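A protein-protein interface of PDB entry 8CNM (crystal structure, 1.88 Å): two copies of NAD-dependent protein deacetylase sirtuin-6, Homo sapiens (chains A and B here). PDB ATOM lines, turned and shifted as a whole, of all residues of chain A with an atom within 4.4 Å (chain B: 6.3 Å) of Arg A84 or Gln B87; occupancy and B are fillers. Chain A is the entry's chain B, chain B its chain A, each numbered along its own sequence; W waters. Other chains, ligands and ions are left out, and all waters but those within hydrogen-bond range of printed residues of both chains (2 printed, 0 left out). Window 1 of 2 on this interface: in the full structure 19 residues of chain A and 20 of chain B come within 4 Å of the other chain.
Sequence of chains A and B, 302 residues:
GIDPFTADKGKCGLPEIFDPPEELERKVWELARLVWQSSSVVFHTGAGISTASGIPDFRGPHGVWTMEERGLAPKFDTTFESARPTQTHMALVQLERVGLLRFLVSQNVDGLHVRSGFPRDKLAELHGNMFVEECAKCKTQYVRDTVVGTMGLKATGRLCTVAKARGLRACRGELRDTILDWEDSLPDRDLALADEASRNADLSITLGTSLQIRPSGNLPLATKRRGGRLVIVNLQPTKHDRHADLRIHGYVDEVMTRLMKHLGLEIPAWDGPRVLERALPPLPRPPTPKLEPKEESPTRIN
O of Ser A53 lies close to O of Ala B52, 3.4 Å away. NE2 of Gln B87 is in hydrogen-bond range of O of Ser A82 (3.0 Å). The guanidinium group (NH2) of Arg A84 sits close to the guanidinium group (NH1) of Arg B84, 3.5 Å away.
The side-chain hydroxyl (OG) of Ser A53 lies within hydrogen-bond range of the backbone carbonyl oxygen (O) of Arg A84, at 2.4 Å.
Arg A84 touches Gln B87.
Arg A84 touches just these residues of chain B: Arg B84 (3.5 Å) and Gln B87 (3.7 Å). Of the printed residues of chain B, Ser A53 touches Ala B52 (3.1 Å). Of the printed residues of chain A, Ala B52 touches Ser A53 (3.1 Å). The nearest residue of chain B that does not touch Arg A84 is Pro B85 (4.9 Å). The nearest residue of chain A that does not touch Gln B87 is Trp A270 (4.1 Å).
Of the 15 printed residues of chain B, 3 touch a printed residue of chain A. Of the 8 printed residues of chain A, 3 touch a printed residue of chain B. Printed residues of chain A that touch a printed residue of chain B: Ser A53, Ser A82 and Arg A84. Among the printed residues, no Asp or Glu carboxylate lies within 4 Å of a Lys or Arg side-chain nitrogen of the other chain.
Arg B84 touches its own counterpart, Arg A84. 4 positions are printed for both chains.
Water W1 lies within hydrogen-bond range of the guanidinium group (NH2) of Arg A84, the guanidinium group (NH1) of Arg B84 and the backbone carbonyl oxygen (O) of Pro A85. Water W2 lies within hydrogen-bond range of OD2 of Asp B253 (2.5 Å), O of Ser A82 (2.9 Å) and NE2 of Gln B87 (3.3 Å).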
ATOM      1  N   SER A  53     -20.019 -16.458  36.902  1.00  0.00           N
ATOM      2  CA  SER A  53     -18.767 -16.396  36.096  1.00  0.00           C
ATOM      3  C   SER A  53     -17.522 -16.637  36.963  1.00  0.00           C
ATOM      4  O   SER A  53     -16.399 -16.519  36.441  1.00  0.00           O
ATOM      5  CB  SER A  53     -18.700 -15.082  35.362  1.00  0.00           C
ATOM      6  OG  SER A  53     -19.502 -15.164  34.192  1.00  0.00           O
ATOM      7  N   SER A  82      -9.754 -13.294  32.668  1.00  0.00           N
ATOM      8  CA  SER A  82     -10.381 -14.481  32.019  1.00  0.00           C
ATOM      9  C   SER A  82     -11.892 -14.591  32.285  1.00  0.00           C
ATOM     10  O   SER A  82     -12.527 -15.504  31.725  1.00  0.00           O
ATOM     11  CB  SER A  82      -9.676 -15.747  32.441  1.00  0.00           C
ATOM     12  OG  SER A  82      -8.342 -15.709  31.965  1.00  0.00           O
ATOM     13  N   ALA A  83     -12.468 -13.745  33.142  1.00  0.00           N
ATOM     14  CA  ALA A  83     -13.905 -13.792  33.483  1.00  0.00           C
ATOM     15  C   ALA A  83     -14.715 -13.552  32.203  1.00  0.00           C
ATOM     16  O   ALA A  83     -14.294 -12.702  31.391  1.00  0.00           O
ATOM     17  CB  ALA A  83     -14.228 -12.766  34.537  1.00  0.00           C
ATOM     18  N   ARG A  84     -15.810 -14.292  32.002  1.00  0.00           N
ATOM     19  CA  ARG A  84     -16.745 -13.998  30.884  1.00  0.00           C
ATOM     20  C   ARG A  84     -17.988 -13.332  31.455  1.00  0.00           C
ATOM     21  O   ARG A  84     -18.476 -13.691  32.526  1.00  0.00           O
ATOM     22  CB  ARG A  84     -17.045 -15.203  29.979  1.00  0.00           C
ATOM     23  CG  ARG A  84     -17.757 -16.392  30.608  1.00  0.00           C
ATOM     24  CD  ARG A  84     -18.544 -17.150  29.538  1.00  0.00           C
ATOM     25  NE  ARG A  84     -19.521 -16.226  28.965  1.00  0.00           N
ATOM     26  CZ  ARG A  84     -19.746 -15.996  27.665  1.00  0.00           C
ATOM     27  NH1 ARG A  84     -19.141 -16.704  26.727  1.00  0.00           N
ATOM     28  NH2 ARG A  84     -20.624 -15.067  27.305  1.00  0.00           N
ATOM     29  N   PRO A  85     -18.576 -12.379  30.700  1.00  0.00           N
ATOM     30  CA  PRO A  85     -19.875 -11.832  31.057  1.00  0.00           C
ATOM     31  C   PRO A  85     -20.887 -12.979  31.145  1.00  0.00           C
ATOM     32  O   PRO A  85     -20.827 -13.911  30.312  1.00  0.00           O
ATOM     33  CB  PRO A  85     -20.244 -10.869  29.926  1.00  0.00           C
ATOM     34  CG  PRO A  85     -18.953 -10.657  29.147  1.00  0.00           C
ATOM     35  CD  PRO A  85     -18.096 -11.879  29.405  1.00  0.00           C
ATOM     36  N   THR A  86     -21.772 -12.890  32.137  1.00  0.00           N
ATOM     37  CA  THR A  86     -22.854 -13.864  32.383  1.00  0.00           C
ATOM     38  C   THR A  86     -23.938 -13.613  31.344  1.00  0.00           C
ATOM     39  O   THR A  86     -23.988 -12.503  30.768  1.00  0.00           O
ATOM     40  CB  THR A  86     -23.448 -13.817  33.807  1.00  0.00           C
ATOM     41  OG1 THR A  86     -24.104 -12.565  34.056  1.00  0.00           O
ATOM     42  CG2 THR A  86     -22.428 -14.063  34.893  1.00  0.00           C
ATOM     43  N   LEU A 112     -16.804  -6.126  33.971  1.00  0.00           N
ATOM     44  CA  LEU A 112     -17.529  -6.994  32.995  1.00  0.00           C
ATOM     45  C   LEU A 112     -18.560  -6.197  32.183  1.00  0.00           C
ATOM     46  O   LEU A 112     -18.664  -6.450  30.983  1.00  0.00           O
ATOM     47  CB  LEU A 112     -18.160  -8.189  33.717  1.00  0.00           C
ATOM     48  CG  LEU A 112     -17.151  -9.254  34.142  1.00  0.00           C
ATOM     49  CD1 LEU A 112     -17.789 -10.343  34.996  1.00  0.00           C
ATOM     50  CD2 LEU A 112     -16.483  -9.867  32.924  1.00  0.00           C
ATOM     51  N   TRP A 270     -21.129 -12.974  22.917  1.00  0.00           N
ATOM     52  CA  TRP A 270     -20.003 -12.152  23.407  1.00  0.00           C
ATOM     53  C   TRP A 270     -18.827 -12.348  22.452  1.00  0.00           C
ATOM     54  O   TRP A 270     -18.324 -13.481  22.375  1.00  0.00           O
ATOM     55  CB  TRP A 270     -19.668 -12.520  24.862  1.00  0.00           C
ATOM     56  CG  TRP A 270     -18.607 -11.649  25.470  1.00  0.00           C
ATOM     57  CD1 TRP A 270     -18.643 -10.283  25.572  1.00  0.00           C
ATOM     58  CD2 TRP A 270     -17.336 -12.055  26.007  1.00  0.00           C
ATOM     59  NE1 TRP A 270     -17.504  -9.822  26.172  1.00  0.00           N
ATOM     60  CE2 TRP A 270     -16.682 -10.883  26.458  1.00  0.00           C
ATOM     61  CE3 TRP A 270     -16.679 -13.280  26.184  1.00  0.00           C
ATOM     62  CZ2 TRP A 270     -15.441 -10.912  27.088  1.00  0.00           C
ATOM     63  CZ3 TRP A 270     -15.454 -13.306  26.799  1.00  0.00           C
ATOM     64  CH2 TRP A 270     -14.827 -12.140  27.246  1.00  0.00           C
ATOM     65  N   ALA B  52     -16.181 -22.185  36.835  1.00  0.00           N
ATOM     66  CA  ALA B  52     -16.333 -20.784  36.337  1.00  0.00           C
ATOM     67  C   ALA B  52     -17.741 -20.534  35.791  1.00  0.00           C
ATOM     68  O   ALA B  52     -18.021 -19.348  35.483  1.00  0.00           O
ATOM     69  CB  ALA B  52     -15.289 -20.483  35.292  1.00  0.00           C
ATOM     70  N   SER B  53     -18.624 -21.542  35.726  1.00  0.00           N
ATOM     71  CA  SER B  53     -20.087 -21.397  35.435  1.00  0.00           C
ATOM     72  C   SER B  53     -20.928 -21.530  36.709  1.00  0.00           C
ATOM     73  O   SER B  53     -22.177 -21.633  36.595  1.00  0.00           O
ATOM     74  CB  SER B  53     -20.498 -22.385  34.388  1.00  0.00           C
ATOM     75  OG  SER B  53     -20.046 -21.947  33.115  1.00  0.00           O
ATOM     76  N   ARG B  84     -24.327 -22.157  32.123  1.00  0.00           N
ATOM     77  CA  ARG B  84     -23.799 -22.018  30.750  1.00  0.00           C
ATOM     78  C   ARG B  84     -22.475 -22.760  30.638  1.00  0.00           C
ATOM     79  O   ARG B  84     -21.636 -22.759  31.548  1.00  0.00           O
ATOM     80  CB  ARG B  84     -23.738 -20.572  30.251  1.00  0.00           C
ATOM     81  CG  ARG B  84     -22.829 -19.619  31.000  1.00  0.00           C
ATOM     82  CD  ARG B  84     -22.387 -18.541  30.030  1.00  0.00           C
ATOM     83  NE  ARG B  84     -21.752 -19.221  28.909  1.00  0.00           N
ATOM     84  CZ  ARG B  84     -21.881 -18.920  27.619  1.00  0.00           C
ATOM     85  NH1 ARG B  84     -22.626 -17.903  27.215  1.00  0.00           N
ATOM     86  NH2 ARG B  84     -21.269 -19.671  26.724  1.00  0.00           N
ATOM     87  N   PRO B  85     -22.235 -23.386  29.464  1.00  0.00           N
ATOM     88  CA  PRO B  85     -20.925 -23.941  29.154  1.00  0.00           C
ATOM     89  C   PRO B  85     -19.876 -22.822  29.280  1.00  0.00           C
ATOM     90  O   PRO B  85     -20.139 -21.690  28.886  1.00  0.00           O
ATOM     91  CB  PRO B  85     -21.020 -24.519  27.738  1.00  0.00           C
ATOM     92  CG  PRO B  85     -22.470 -24.334  27.300  1.00  0.00           C
ATOM     93  CD  PRO B  85     -23.204 -23.584  28.393  1.00  0.00           C
ATOM     94  N   THR B  86     -18.724 -23.148  29.862  1.00  0.00           N
ATOM     95  CA  THR B  86     -17.567 -22.236  30.018  1.00  0.00           C
ATOM     96  C   THR B  86     -16.845 -22.104  28.675  1.00  0.00           C
ATOM     97  O   THR B  86     -17.140 -22.893  27.736  1.00  0.00           O
ATOM     98  CB  THR B  86     -16.530 -22.693  31.065  1.00  0.00           C
ATOM     99  OG1 THR B  86     -15.901 -23.902  30.604  1.00  0.00           O
ATOM    100  CG2 THR B  86     -17.137 -22.861  32.435  1.00  0.00           C
ATOM    101  N   GLN B  87     -15.937 -21.133  28.613  1.00  0.00           N
ATOM    102  CA  GLN B  87     -14.947 -20.935  27.517  1.00  0.00           C
ATOM    103  C   GLN B  87     -14.264 -22.282  27.232  1.00  0.00           C
ATOM    104  O   GLN B  87     -14.177 -22.678  26.066  1.00  0.00           O
ATOM    105  CB  GLN B  87     -14.011 -19.807  27.928  1.00  0.00           C
ATOM    106  CG  GLN B  87     -14.732 -18.467  27.909  1.00  0.00           C
ATOM    107  CD  GLN B  87     -13.918 -17.383  28.569  1.00  0.00           C
ATOM    108  OE1 GLN B  87     -13.231 -16.612  27.907  1.00  0.00           O
ATOM    109  NE2 GLN B  87     -13.988 -17.325  29.884  1.00  0.00           N
ATOM    110  N   THR B  88     -13.956 -23.013  28.279  1.00  0.00           N
ATOM    111  CA  THR B  88     -13.274 -24.327  28.175  1.00  0.00           C
ATOM    112  C   THR B  88     -14.203 -25.259  27.436  1.00  0.00           C
ATOM    113  O   THR B  88     -13.746 -25.746  26.400  1.00  0.00           O
ATOM    114  CB  THR B  88     -12.845 -24.883  29.530  1.00  0.00           C
ATOM    115  OG1 THR B  88     -11.764 -24.057  29.927  1.00  0.00           O
ATOM    116  CG2 THR B  88     -12.341 -26.310  29.453  1.00  0.00           C
ATOM    117  N   HIS B  89     -15.476 -25.352  27.861  1.00  0.00           N
ATOM    118  CA  HIS B  89     -16.514 -26.189  27.206  1.00  0.00           C
ATOM    119  C   HIS B  89     -16.555 -25.870  25.707  1.00  0.00           C
ATOM    120  O   HIS B  89     -16.554 -26.794  24.868  1.00  0.00           O
ATOM    121  CB  HIS B  89     -17.902 -26.062  27.872  1.00  0.00           C
ATOM    122  CG  HIS B  89     -18.040 -26.751  29.183  1.00  0.00           C
ATOM    123  ND1 HIS B  89     -17.843 -26.098  30.365  1.00  0.00           N
ATOM    124  CD2 HIS B  89     -18.431 -28.006  29.508  1.00  0.00           C
ATOM    125  CE1 HIS B  89     -18.034 -26.925  31.371  1.00  0.00           C
ATOM    126  NE2 HIS B  89     -18.352 -28.132  30.861  1.00  0.00           N
ATOM    127  N   MET B  90     -16.663 -24.588  25.354  1.00  0.00           N
ATOM    128  CA  MET B  90     -16.869 -24.167  23.956  1.00  0.00           C
ATOM    129  C   MET B  90     -15.578 -24.380  23.140  1.00  0.00           C
ATOM    130  O   MET B  90     -15.703 -24.787  21.951  1.00  0.00           O
ATOM    131  CB  MET B  90     -17.396 -22.715  23.937  1.00  0.00           C
ATOM    132  CG  MET B  90     -18.772 -22.566  24.580  1.00  0.00           C
ATOM    133  SD  MET B  90     -20.049 -23.863  24.202  1.00  0.00           S
ATOM    134  CE  MET B  90     -20.276 -23.630  22.442  1.00  0.00           C
ATOM    135  N   ALA B  91     -14.377 -24.239  23.725  1.00  0.00           N
ATOM    136  CA  ALA B  91     -13.098 -24.487  23.016  1.00  0.00           C
ATOM    137  C   ALA B  91     -13.063 -25.964  22.617  1.00  0.00           C
ATOM    138  O   ALA B  91     -12.612 -26.249  21.498  1.00  0.00           O
ATOM    139  CB  ALA B  91     -11.895 -24.178  23.864  1.00  0.00           C
ATOM    140  N   LEU B  92     -13.632 -26.826  23.460  1.00  0.00           N
ATOM    141  CA  LEU B  92     -13.570 -28.301  23.233  1.00  0.00           C
ATOM    142  C   LEU B  92     -14.516 -28.659  22.082  1.00  0.00           C
ATOM    143  O   LEU B  92     -14.212 -29.645  21.322  1.00  0.00           O
ATOM    144  CB  LEU B  92     -13.908 -29.037  24.530  1.00  0.00           C
ATOM    145  CG  LEU B  92     -12.838 -28.945  25.622  1.00  0.00           C
ATOM    146  CD1 LEU B  92     -13.385 -29.419  26.961  1.00  0.00           C
ATOM    147  CD2 LEU B  92     -11.585 -29.710  25.211  1.00  0.00           C
ATOM    148  N   ASP B 253      -9.746 -21.941  31.941  1.00  0.00           N
ATOM    149  CA  ASP B 253     -10.266 -21.013  30.905  1.00  0.00           C
ATOM    150  C   ASP B 253      -9.117 -20.165  30.364  1.00  0.00           C
ATOM    151  O   ASP B 253      -9.154 -19.894  29.160  1.00  0.00           O
ATOM    152  CB  ASP B 253     -11.390 -20.101  31.379  1.00  0.00           C
ATOM    153  CG  ASP B 253     -12.735 -20.763  31.434  1.00  0.00           C
ATOM    154  OD1 ASP B 253     -12.914 -21.913  30.825  1.00  0.00           O
ATOM    155  OD2 ASP B 253     -13.593 -20.162  32.093  1.00  0.00           O
ATOM    156  N   MET B 256      -7.039 -22.473  28.126  1.00  0.00           N
ATOM    157  CA  MET B 256      -7.687 -22.942  26.882  1.00  0.00           C
ATOM    158  C   MET B 256      -7.873 -21.746  25.953  1.00  0.00           C
ATOM    159  O   MET B 256      -7.689 -21.933  24.791  1.00  0.00           O
ATOM    160  CB  MET B 256      -9.007 -23.661  27.122  1.00  0.00           C
ATOM    161  CG  MET B 256      -8.851 -24.989  27.815  1.00  0.00           C
ATOM    162  SD  MET B 256      -7.861 -26.158  26.820  1.00  0.00           S
ATOM    163  CE  MET B 256      -9.043 -26.485  25.526  1.00  0.00           C
ATOM    164  N   THR B 257      -8.100 -20.525  26.460  1.00  0.00           N
ATOM    165  CA  THR B 257      -8.210 -19.333  25.580  1.00  0.00           C
ATOM    166  C   THR B 257      -6.850 -18.982  24.934  1.00  0.00           C
ATOM    167  O   THR B 257      -6.849 -18.588  23.742  1.00  0.00           O
ATOM    168  CB  THR B 257      -8.848 -18.153  26.340  1.00  0.00           C
ATOM    169  OG1 THR B 257      -8.071 -17.821  27.478  1.00  0.00           O
ATOM    170  CG2 THR B 257     -10.239 -18.436  26.836  1.00  0.00           C
ATOM    171  N   ILE B 267     -13.229 -19.289  19.772  1.00  0.00           N
ATOM    172  CA  ILE B 267     -14.157 -20.038  20.656  1.00  0.00           C
ATOM    173  C   ILE B 267     -15.559 -19.689  20.191  1.00  0.00           C
ATOM    174  O   ILE B 267     -15.953 -18.523  20.227  1.00  0.00           O
ATOM    175  CB  ILE B 267     -13.928 -19.722  22.142  1.00  0.00           C
ATOM    176  CG1 ILE B 267     -12.524 -20.153  22.579  1.00  0.00           C
ATOM    177  CG2 ILE B 267     -15.046 -20.358  22.971  1.00  0.00           C
ATOM    178  CD1 ILE B 267     -12.200 -19.896  24.036  1.00  0.00           C
HETATM  179  O   HOH W   1     -22.729 -15.253  28.446  1.00  0.00           O
HETATM  180  O   HOH W   2     -13.455 -17.899  33.099  1.00  0.00           O
